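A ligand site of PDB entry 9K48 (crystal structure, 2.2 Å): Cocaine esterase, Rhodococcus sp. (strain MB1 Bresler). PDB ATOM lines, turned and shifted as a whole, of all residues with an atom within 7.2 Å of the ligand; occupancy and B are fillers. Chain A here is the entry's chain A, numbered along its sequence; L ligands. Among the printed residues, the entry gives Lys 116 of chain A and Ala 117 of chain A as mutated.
The backbone NH (N) of Tyr 118 lies within hydrogen-bond range of an oxygen (O2) of the ligand (3.1 Å).
OH of Tyr 44 sits at hydrogen-bond distance from O2 of the ligand (2.5 Å).
A ring nitrogen (NE2) of His 287 sits at hydrogen-bond distance from an oxygen (O1) of the ligand (2.7 Å).
The backbone NH of Trp 151 sits at hydrogen-bond distance from the backbone carbonyl oxygen of Leu 146 (3.2 Å).
OH of Tyr 118 is in hydrogen-bond range of N of His 87.
A ring nitrogen (NE2) of His 87 sits at hydrogen-bond distance from the indole nitrogen (NE1) of Trp 151 (3.0 Å).
NZ of Lys 116 lies within hydrogen-bond range of O of His 287 (2.7 Å).
N of Ala 117 sits close to O of Met 141 (3.5 Å).
OH of Tyr 44 is in hydrogen-bond range of NE1 of Trp 166, 2.9 Å away.
Merely in contact with the ligand: Ala 117, Trp 166, Pro 150, Trp 151, Phe 408, Phe 261 and Leu 407.
Within 4 Å of the ligand: Tyr 44, Ala 117, Tyr 118, Pro 150, Trp 151, Trp 166, Phe 261, His 287, Leu 407 and Phe 408.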
ATOM      1  N   PRO A  43       9.801 -17.650  -6.637  1.00  0.00           N
ATOM      2  CA  PRO A  43       9.831 -18.040  -8.044  1.00  0.00           C
ATOM      3  C   PRO A  43       8.463 -18.059  -8.706  1.00  0.00           C
ATOM      4  O   PRO A  43       8.367 -18.493  -9.859  1.00  0.00           O
ATOM      5  CB  PRO A  43      10.422 -19.462  -7.968  1.00  0.00           C
ATOM      6  CG  PRO A  43       9.785 -20.015  -6.707  1.00  0.00           C
ATOM      7  CD  PRO A  43       9.712 -18.827  -5.751  1.00  0.00           C
ATOM      8  N   TYR A  44       7.405 -17.641  -8.022  1.00  0.00           N
ATOM      9  CA  TYR A  44       6.048 -17.791  -8.542  1.00  0.00           C
ATOM     10  C   TYR A  44       5.364 -16.442  -8.751  1.00  0.00           C
ATOM     11  O   TYR A  44       4.137 -16.333  -8.612  1.00  0.00           O
ATOM     12  CB  TYR A  44       5.207 -18.670  -7.605  1.00  0.00           C
ATOM     13  CG  TYR A  44       5.870 -19.964  -7.171  1.00  0.00           C
ATOM     14  CD1 TYR A  44       6.177 -20.953  -8.097  1.00  0.00           C
ATOM     15  CD2 TYR A  44       6.152 -20.203  -5.837  1.00  0.00           C
ATOM     16  CE1 TYR A  44       6.768 -22.141  -7.701  1.00  0.00           C
ATOM     17  CE2 TYR A  44       6.732 -21.366  -5.428  1.00  0.00           C
ATOM     18  CZ  TYR A  44       7.046 -22.334  -6.356  1.00  0.00           C
ATOM     19  OH  TYR A  44       7.649 -23.491  -5.946  1.00  0.00           O
ATOM     20  N   HIS A  87      17.573 -23.472  -7.673  1.00  0.00           N
ATOM     21  CA  HIS A  87      18.485 -23.588  -6.532  1.00  0.00           C
ATOM     22  C   HIS A  87      19.882 -23.013  -6.753  1.00  0.00           C
ATOM     23  O   HIS A  87      20.453 -22.435  -5.829  1.00  0.00           O
ATOM     24  CB  HIS A  87      18.664 -25.047  -6.093  1.00  0.00           C
ATOM     25  CG  HIS A  87      17.389 -25.795  -5.858  1.00  0.00           C
ATOM     26  ND1 HIS A  87      16.288 -25.236  -5.240  1.00  0.00           N
ATOM     27  CD2 HIS A  87      17.040 -27.084  -6.138  1.00  0.00           C
ATOM     28  CE1 HIS A  87      15.326 -26.137  -5.159  1.00  0.00           C
ATOM     29  NE2 HIS A  87      15.763 -27.268  -5.700  1.00  0.00           N
ATOM     30  N   LYS A 116       7.238 -19.964   2.429  1.00  0.00           N
ATOM     31  CA  LYS A 116       6.962 -21.396   2.506  1.00  0.00           C
ATOM     32  C   LYS A 116       7.603 -22.155   1.345  1.00  0.00           C
ATOM     33  O   LYS A 116       7.649 -21.655   0.215  1.00  0.00           O
ATOM     34  CB  LYS A 116       5.436 -21.604   2.499  1.00  0.00           C
ATOM     35  CG  LYS A 116       4.967 -23.045   2.497  1.00  0.00           C
ATOM     36  CD  LYS A 116       3.443 -23.130   2.491  1.00  0.00           C
ATOM     37  CE  LYS A 116       2.944 -24.558   2.777  1.00  0.00           C
ATOM     38  NZ  LYS A 116       2.921 -25.470   1.599  1.00  0.00           N
ATOM     39  N   ALA A 117       8.075 -23.371   1.627  1.00  0.00           N
ATOM     40  CA  ALA A 117       8.581 -24.282   0.607  1.00  0.00           C
ATOM     41  C   ALA A 117       9.799 -23.725  -0.132  1.00  0.00           C
ATOM     42  O   ALA A 117      10.838 -23.446   0.484  1.00  0.00           O
ATOM     43  CB  ALA A 117       7.462 -24.644  -0.377  1.00  0.00           C
ATOM     44  N   TYR A 118       9.691 -23.540  -1.453  1.00  0.00           N
ATOM     45  CA  TYR A 118      10.791 -22.920  -2.204  1.00  0.00           C
ATOM     46  C   TYR A 118      11.148 -21.549  -1.627  1.00  0.00           C
ATOM     47  O   TYR A 118      12.328 -21.174  -1.609  1.00  0.00           O
ATOM     48  CB  TYR A 118      10.439 -22.805  -3.684  1.00  0.00           C
ATOM     49  CG  TYR A 118      11.614 -22.582  -4.613  1.00  0.00           C
ATOM     50  CD1 TYR A 118      12.258 -21.343  -4.693  1.00  0.00           C
ATOM     51  CD2 TYR A 118      12.078 -23.609  -5.435  1.00  0.00           C
ATOM     52  CE1 TYR A 118      13.338 -21.137  -5.560  1.00  0.00           C
ATOM     53  CE2 TYR A 118      13.155 -23.412  -6.297  1.00  0.00           C
ATOM     54  CZ  TYR A 118      13.776 -22.183  -6.364  1.00  0.00           C
ATOM     55  OH  TYR A 118      14.836 -22.003  -7.222  1.00  0.00           O
ATOM     56  N   LEU A 119      10.157 -20.794  -1.131  1.00  0.00           N
ATOM     57  CA  LEU A 119      10.421 -19.538  -0.449  1.00  0.00           C
ATOM     58  C   LEU A 119      10.983 -19.731   0.963  1.00  0.00           C
ATOM     59  O   LEU A 119      11.478 -18.759   1.557  1.00  0.00           O
ATOM     60  CB  LEU A 119       9.139 -18.691  -0.391  1.00  0.00           C
ATOM     61  CG  LEU A 119       8.521 -18.147  -1.687  1.00  0.00           C
ATOM     62  CD1 LEU A 119       7.979 -19.255  -2.582  1.00  0.00           C
ATOM     63  CD2 LEU A 119       7.392 -17.188  -1.371  1.00  0.00           C
ATOM     64  N   GLY A 120      10.950 -20.946   1.496  1.00  0.00           N
ATOM     65  CA  GLY A 120      11.665 -21.255   2.724  1.00  0.00           C
ATOM     66  C   GLY A 120      13.075 -21.736   2.455  1.00  0.00           C
ATOM     67  O   GLY A 120      14.008 -21.406   3.194  1.00  0.00           O
ATOM     68  N   VAL A 121      13.244 -22.534   1.403  1.00  0.00           N
ATOM     69  CA  VAL A 121      14.579 -22.937   0.958  1.00  0.00           C
ATOM     70  C   VAL A 121      15.437 -21.705   0.697  1.00  0.00           C
ATOM     71  O   VAL A 121      16.596 -21.638   1.135  1.00  0.00           O
ATOM     72  CB  VAL A 121      14.491 -23.833  -0.280  1.00  0.00           C
ATOM     73  CG1 VAL A 121      15.894 -24.086  -0.879  1.00  0.00           C
ATOM     74  CG2 VAL A 121      13.804 -25.148   0.059  1.00  0.00           C
ATOM     75  N   MET A 141       7.736 -24.950   6.199  1.00  0.00           N
ATOM     76  CA  MET A 141       7.542 -26.206   5.471  1.00  0.00           C
ATOM     77  C   MET A 141       8.565 -26.351   4.345  1.00  0.00           C
ATOM     78  O   MET A 141       8.229 -26.462   3.167  1.00  0.00           O
ATOM     79  CB  MET A 141       6.095 -26.325   4.997  1.00  0.00           C
ATOM     80  CG  MET A 141       5.169 -26.323   6.210  1.00  0.00           C
ATOM     81  SD  MET A 141       3.411 -26.428   5.979  1.00  0.00           S
ATOM     82  CE  MET A 141       2.946 -24.756   6.340  1.00  0.00           C
ATOM     83  N   LEU A 146      18.360 -30.377  -0.404  1.00  0.00           N
ATOM     84  CA  LEU A 146      17.402 -30.551  -1.498  1.00  0.00           C
ATOM     85  C   LEU A 146      17.306 -31.999  -1.969  1.00  0.00           C
ATOM     86  O   LEU A 146      16.267 -32.386  -2.524  1.00  0.00           O
ATOM     87  CB  LEU A 146      17.753 -29.632  -2.664  1.00  0.00           C
ATOM     88  CG  LEU A 146      17.485 -28.132  -2.479  1.00  0.00           C
ATOM     89  CD1 LEU A 146      16.090 -27.909  -1.902  1.00  0.00           C
ATOM     90  CD2 LEU A 146      18.546 -27.481  -1.605  1.00  0.00           C
ATOM     91  N   ALA A 149      14.946 -33.543   0.837  1.00  0.00           N
ATOM     92  CA  ALA A 149      13.600 -33.066   0.530  1.00  0.00           C
ATOM     93  C   ALA A 149      13.745 -31.804  -0.314  1.00  0.00           C
ATOM     94  O   ALA A 149      14.481 -30.892   0.048  1.00  0.00           O
ATOM     95  CB  ALA A 149      12.777 -32.793   1.807  1.00  0.00           C
ATOM     96  N   PRO A 150      13.011 -31.730  -1.439  1.00  0.00           N
ATOM     97  CA  PRO A 150      11.933 -32.643  -1.803  1.00  0.00           C
ATOM     98  C   PRO A 150      12.240 -33.595  -2.952  1.00  0.00           C
ATOM     99  O   PRO A 150      11.309 -34.253  -3.387  1.00  0.00           O
ATOM    100  CB  PRO A 150      10.834 -31.674  -2.228  1.00  0.00           C
ATOM    101  CG  PRO A 150      11.624 -30.558  -2.938  1.00  0.00           C
ATOM    102  CD  PRO A 150      13.006 -30.523  -2.301  1.00  0.00           C
ATOM    103  N   TRP A 151      13.475 -33.692  -3.445  1.00  0.00           N
ATOM    104  CA  TRP A 151      13.628 -34.413  -4.703  1.00  0.00           C
ATOM    105  C   TRP A 151      13.905 -35.906  -4.536  1.00  0.00           C
ATOM    106  O   TRP A 151      13.394 -36.722  -5.308  1.00  0.00           O
ATOM    107  CB  TRP A 151      14.719 -33.754  -5.567  1.00  0.00           C
ATOM    108  CG  TRP A 151      14.435 -32.301  -5.780  1.00  0.00           C
ATOM    109  CD1 TRP A 151      15.285 -31.270  -5.544  1.00  0.00           C
ATOM    110  CD2 TRP A 151      13.198 -31.718  -6.217  1.00  0.00           C
ATOM    111  NE1 TRP A 151      14.668 -30.070  -5.820  1.00  0.00           N
ATOM    112  CE2 TRP A 151      13.383 -30.316  -6.248  1.00  0.00           C
ATOM    113  CE3 TRP A 151      11.958 -32.237  -6.612  1.00  0.00           C
ATOM    114  CZ2 TRP A 151      12.377 -29.428  -6.644  1.00  0.00           C
ATOM    115  CZ3 TRP A 151      10.956 -31.365  -7.011  1.00  0.00           C
ATOM    116  CH2 TRP A 151      11.175 -29.967  -7.015  1.00  0.00           C
ATOM    117  N   ALA A 162       6.806 -35.778  -6.906  1.00  0.00           N
ATOM    118  CA  ALA A 162       7.214 -34.436  -6.555  1.00  0.00           C
ATOM    119  C   ALA A 162       7.926 -33.761  -7.729  1.00  0.00           C
ATOM    120  O   ALA A 162       7.623 -32.615  -8.083  1.00  0.00           O
ATOM    121  CB  ALA A 162       8.116 -34.461  -5.320  1.00  0.00           C
ATOM    122  N   LEU A 163       8.860 -34.490  -8.342  1.00  0.00           N
ATOM    123  CA  LEU A 163       9.618 -33.968  -9.467  1.00  0.00           C
ATOM    124  C   LEU A 163       8.703 -33.584 -10.628  1.00  0.00           C
ATOM    125  O   LEU A 163       8.734 -32.449 -11.115  1.00  0.00           O
ATOM    126  CB  LEU A 163      10.645 -34.997  -9.914  1.00  0.00           C
ATOM    127  CG  LEU A 163      11.512 -34.546 -11.080  1.00  0.00           C
ATOM    128  CD1 LEU A 163      12.291 -33.291 -10.664  1.00  0.00           C
ATOM    129  CD2 LEU A 163      12.456 -35.667 -11.498  1.00  0.00           C
ATOM    130  N   TRP A 166       5.967 -30.753  -9.807  1.00  0.00           N
ATOM    131  CA  TRP A 166       6.533 -29.405  -9.698  1.00  0.00           C
ATOM    132  C   TRP A 166       7.053 -28.891 -11.032  1.00  0.00           C
ATOM    133  O   TRP A 166       6.857 -27.722 -11.360  1.00  0.00           O
ATOM    134  CB  TRP A 166       7.653 -29.359  -8.653  1.00  0.00           C
ATOM    135  CG  TRP A 166       8.150 -27.933  -8.342  1.00  0.00           C
ATOM    136  CD1 TRP A 166       7.524 -26.988  -7.566  1.00  0.00           C
ATOM    137  CD2 TRP A 166       9.385 -27.334  -8.765  1.00  0.00           C
ATOM    138  NE1 TRP A 166       8.292 -25.841  -7.489  1.00  0.00           N
ATOM    139  CE2 TRP A 166       9.436 -26.033  -8.221  1.00  0.00           C
ATOM    140  CE3 TRP A 166      10.445 -27.770  -9.571  1.00  0.00           C
ATOM    141  CZ2 TRP A 166      10.508 -25.171  -8.446  1.00  0.00           C
ATOM    142  CZ3 TRP A 166      11.507 -26.905  -9.794  1.00  0.00           C
ATOM    143  CH2 TRP A 166      11.532 -25.622  -9.232  1.00  0.00           C
ATOM    144  N   LEU A 169       4.202 -27.640 -13.123  1.00  0.00           N
ATOM    145  CA  LEU A 169       3.689 -26.330 -12.696  1.00  0.00           C
ATOM    146  C   LEU A 169       4.627 -25.214 -13.118  1.00  0.00           C
ATOM    147  O   LEU A 169       4.179 -24.104 -13.419  1.00  0.00           O
ATOM    148  CB  LEU A 169       3.492 -26.289 -11.182  1.00  0.00           C
ATOM    149  CG  LEU A 169       2.352 -27.101 -10.572  1.00  0.00           C
ATOM    150  CD1 LEU A 169       2.611 -27.329  -9.082  1.00  0.00           C
ATOM    151  CD2 LEU A 169       0.988 -26.424 -10.809  1.00  0.00           C
ATOM    152  N   PHE A 261       8.231 -31.813   3.011  1.00  0.00           N
ATOM    153  CA  PHE A 261       9.468 -31.333   3.607  1.00  0.00           C
ATOM    154  C   PHE A 261       9.620 -31.653   5.098  1.00  0.00           C
ATOM    155  O   PHE A 261      10.614 -31.231   5.707  1.00  0.00           O
ATOM    156  CB  PHE A 261       9.576 -29.806   3.434  1.00  0.00           C
ATOM    157  CG  PHE A 261       9.507 -29.332   2.008  1.00  0.00           C
ATOM    158  CD1 PHE A 261       8.280 -29.143   1.386  1.00  0.00           C
ATOM    159  CD2 PHE A 261      10.663 -29.045   1.298  1.00  0.00           C
ATOM    160  CE1 PHE A 261       8.212 -28.678   0.096  1.00  0.00           C
ATOM    161  CE2 PHE A 261      10.601 -28.588  -0.002  1.00  0.00           C
ATOM    162  CZ  PHE A 261       9.366 -28.400  -0.608  1.00  0.00           C
ATOM    163  N   HIS A 287       1.206 -30.353   1.993  1.00  0.00           N
ATOM    164  CA  HIS A 287       1.795 -29.189   1.342  1.00  0.00           C
ATOM    165  C   HIS A 287       0.733 -28.283   0.763  1.00  0.00           C
ATOM    166  O   HIS A 287       0.858 -27.050   0.823  1.00  0.00           O
ATOM    167  CB  HIS A 287       2.769 -29.636   0.259  1.00  0.00           C
ATOM    168  CG  HIS A 287       3.104 -28.571  -0.746  1.00  0.00           C
ATOM    169  ND1 HIS A 287       2.336 -28.352  -1.871  1.00  0.00           N
ATOM    170  CD2 HIS A 287       4.142 -27.703  -0.808  1.00  0.00           C
ATOM    171  CE1 HIS A 287       2.878 -27.368  -2.572  1.00  0.00           C
ATOM    172  NE2 HIS A 287       3.975 -26.956  -1.954  1.00  0.00           N
ATOM    173  N   LEU A 407       2.974 -34.794  -2.628  1.00  0.00           N
ATOM    174  CA  LEU A 407       2.982 -33.364  -2.917  1.00  0.00           C
ATOM    175  C   LEU A 407       1.953 -32.971  -3.966  1.00  0.00           C
ATOM    176  O   LEU A 407       1.135 -32.070  -3.736  1.00  0.00           O
ATOM    177  CB  LEU A 407       4.377 -32.907  -3.357  1.00  0.00           C
ATOM    178  CG  LEU A 407       5.387 -32.780  -2.217  1.00  0.00           C
ATOM    179  CD1 LEU A 407       6.799 -32.551  -2.735  1.00  0.00           C
ATOM    180  CD2 LEU A 407       4.986 -31.617  -1.348  1.00  0.00           C
ATOM    181  N   PHE A 408       1.961 -33.621  -5.123  1.00  0.00           N
ATOM    182  CA  PHE A 408       1.082 -33.241  -6.222  1.00  0.00           C
ATOM    183  C   PHE A 408       0.177 -34.359  -6.689  1.00  0.00           C
ATOM    184  O   PHE A 408      -0.925 -34.070  -7.180  1.00  0.00           O
ATOM    185  CB  PHE A 408       1.910 -32.720  -7.392  1.00  0.00           C
ATOM    186  CG  PHE A 408       2.809 -31.592  -7.023  1.00  0.00           C
ATOM    187  CD1 PHE A 408       2.282 -30.357  -6.681  1.00  0.00           C
ATOM    188  CD2 PHE A 408       4.179 -31.777  -6.972  1.00  0.00           C
ATOM    189  CE1 PHE A 408       3.105 -29.322  -6.319  1.00  0.00           C
ATOM    190  CE2 PHE A 408       5.003 -30.734  -6.616  1.00  0.00           C
ATOM    191  CZ  PHE A 408       4.471 -29.509  -6.290  1.00  0.00           C
HETATM  192  C1  LIG L   1       6.864 -25.218  -3.558  1.00  0.00           C
HETATM  193  O1  LIG L   1       5.622 -25.245  -3.314  1.00  0.00           O
HETATM  194  O2  LIG L   1       7.492 -24.130  -3.499  1.00  0.00           O
HETATM  195  C2  LIG L   1       7.554 -26.512  -3.881  1.00  0.00           C
HETATM  196  C3  LIG L   1       8.890 -26.516  -4.244  1.00  0.00           C
HETATM  197  C4  LIG L   1       9.517 -27.723  -4.538  1.00  0.00           C
HETATM  198  C5  LIG L   1       8.801 -28.916  -4.474  1.00  0.00           C
HETATM  199  C6  LIG L   1       7.461 -28.899  -4.094  1.00  0.00           C
HETATM  200  C7  LIG L   1       6.832 -27.699  -3.795  1.00  0.00           C
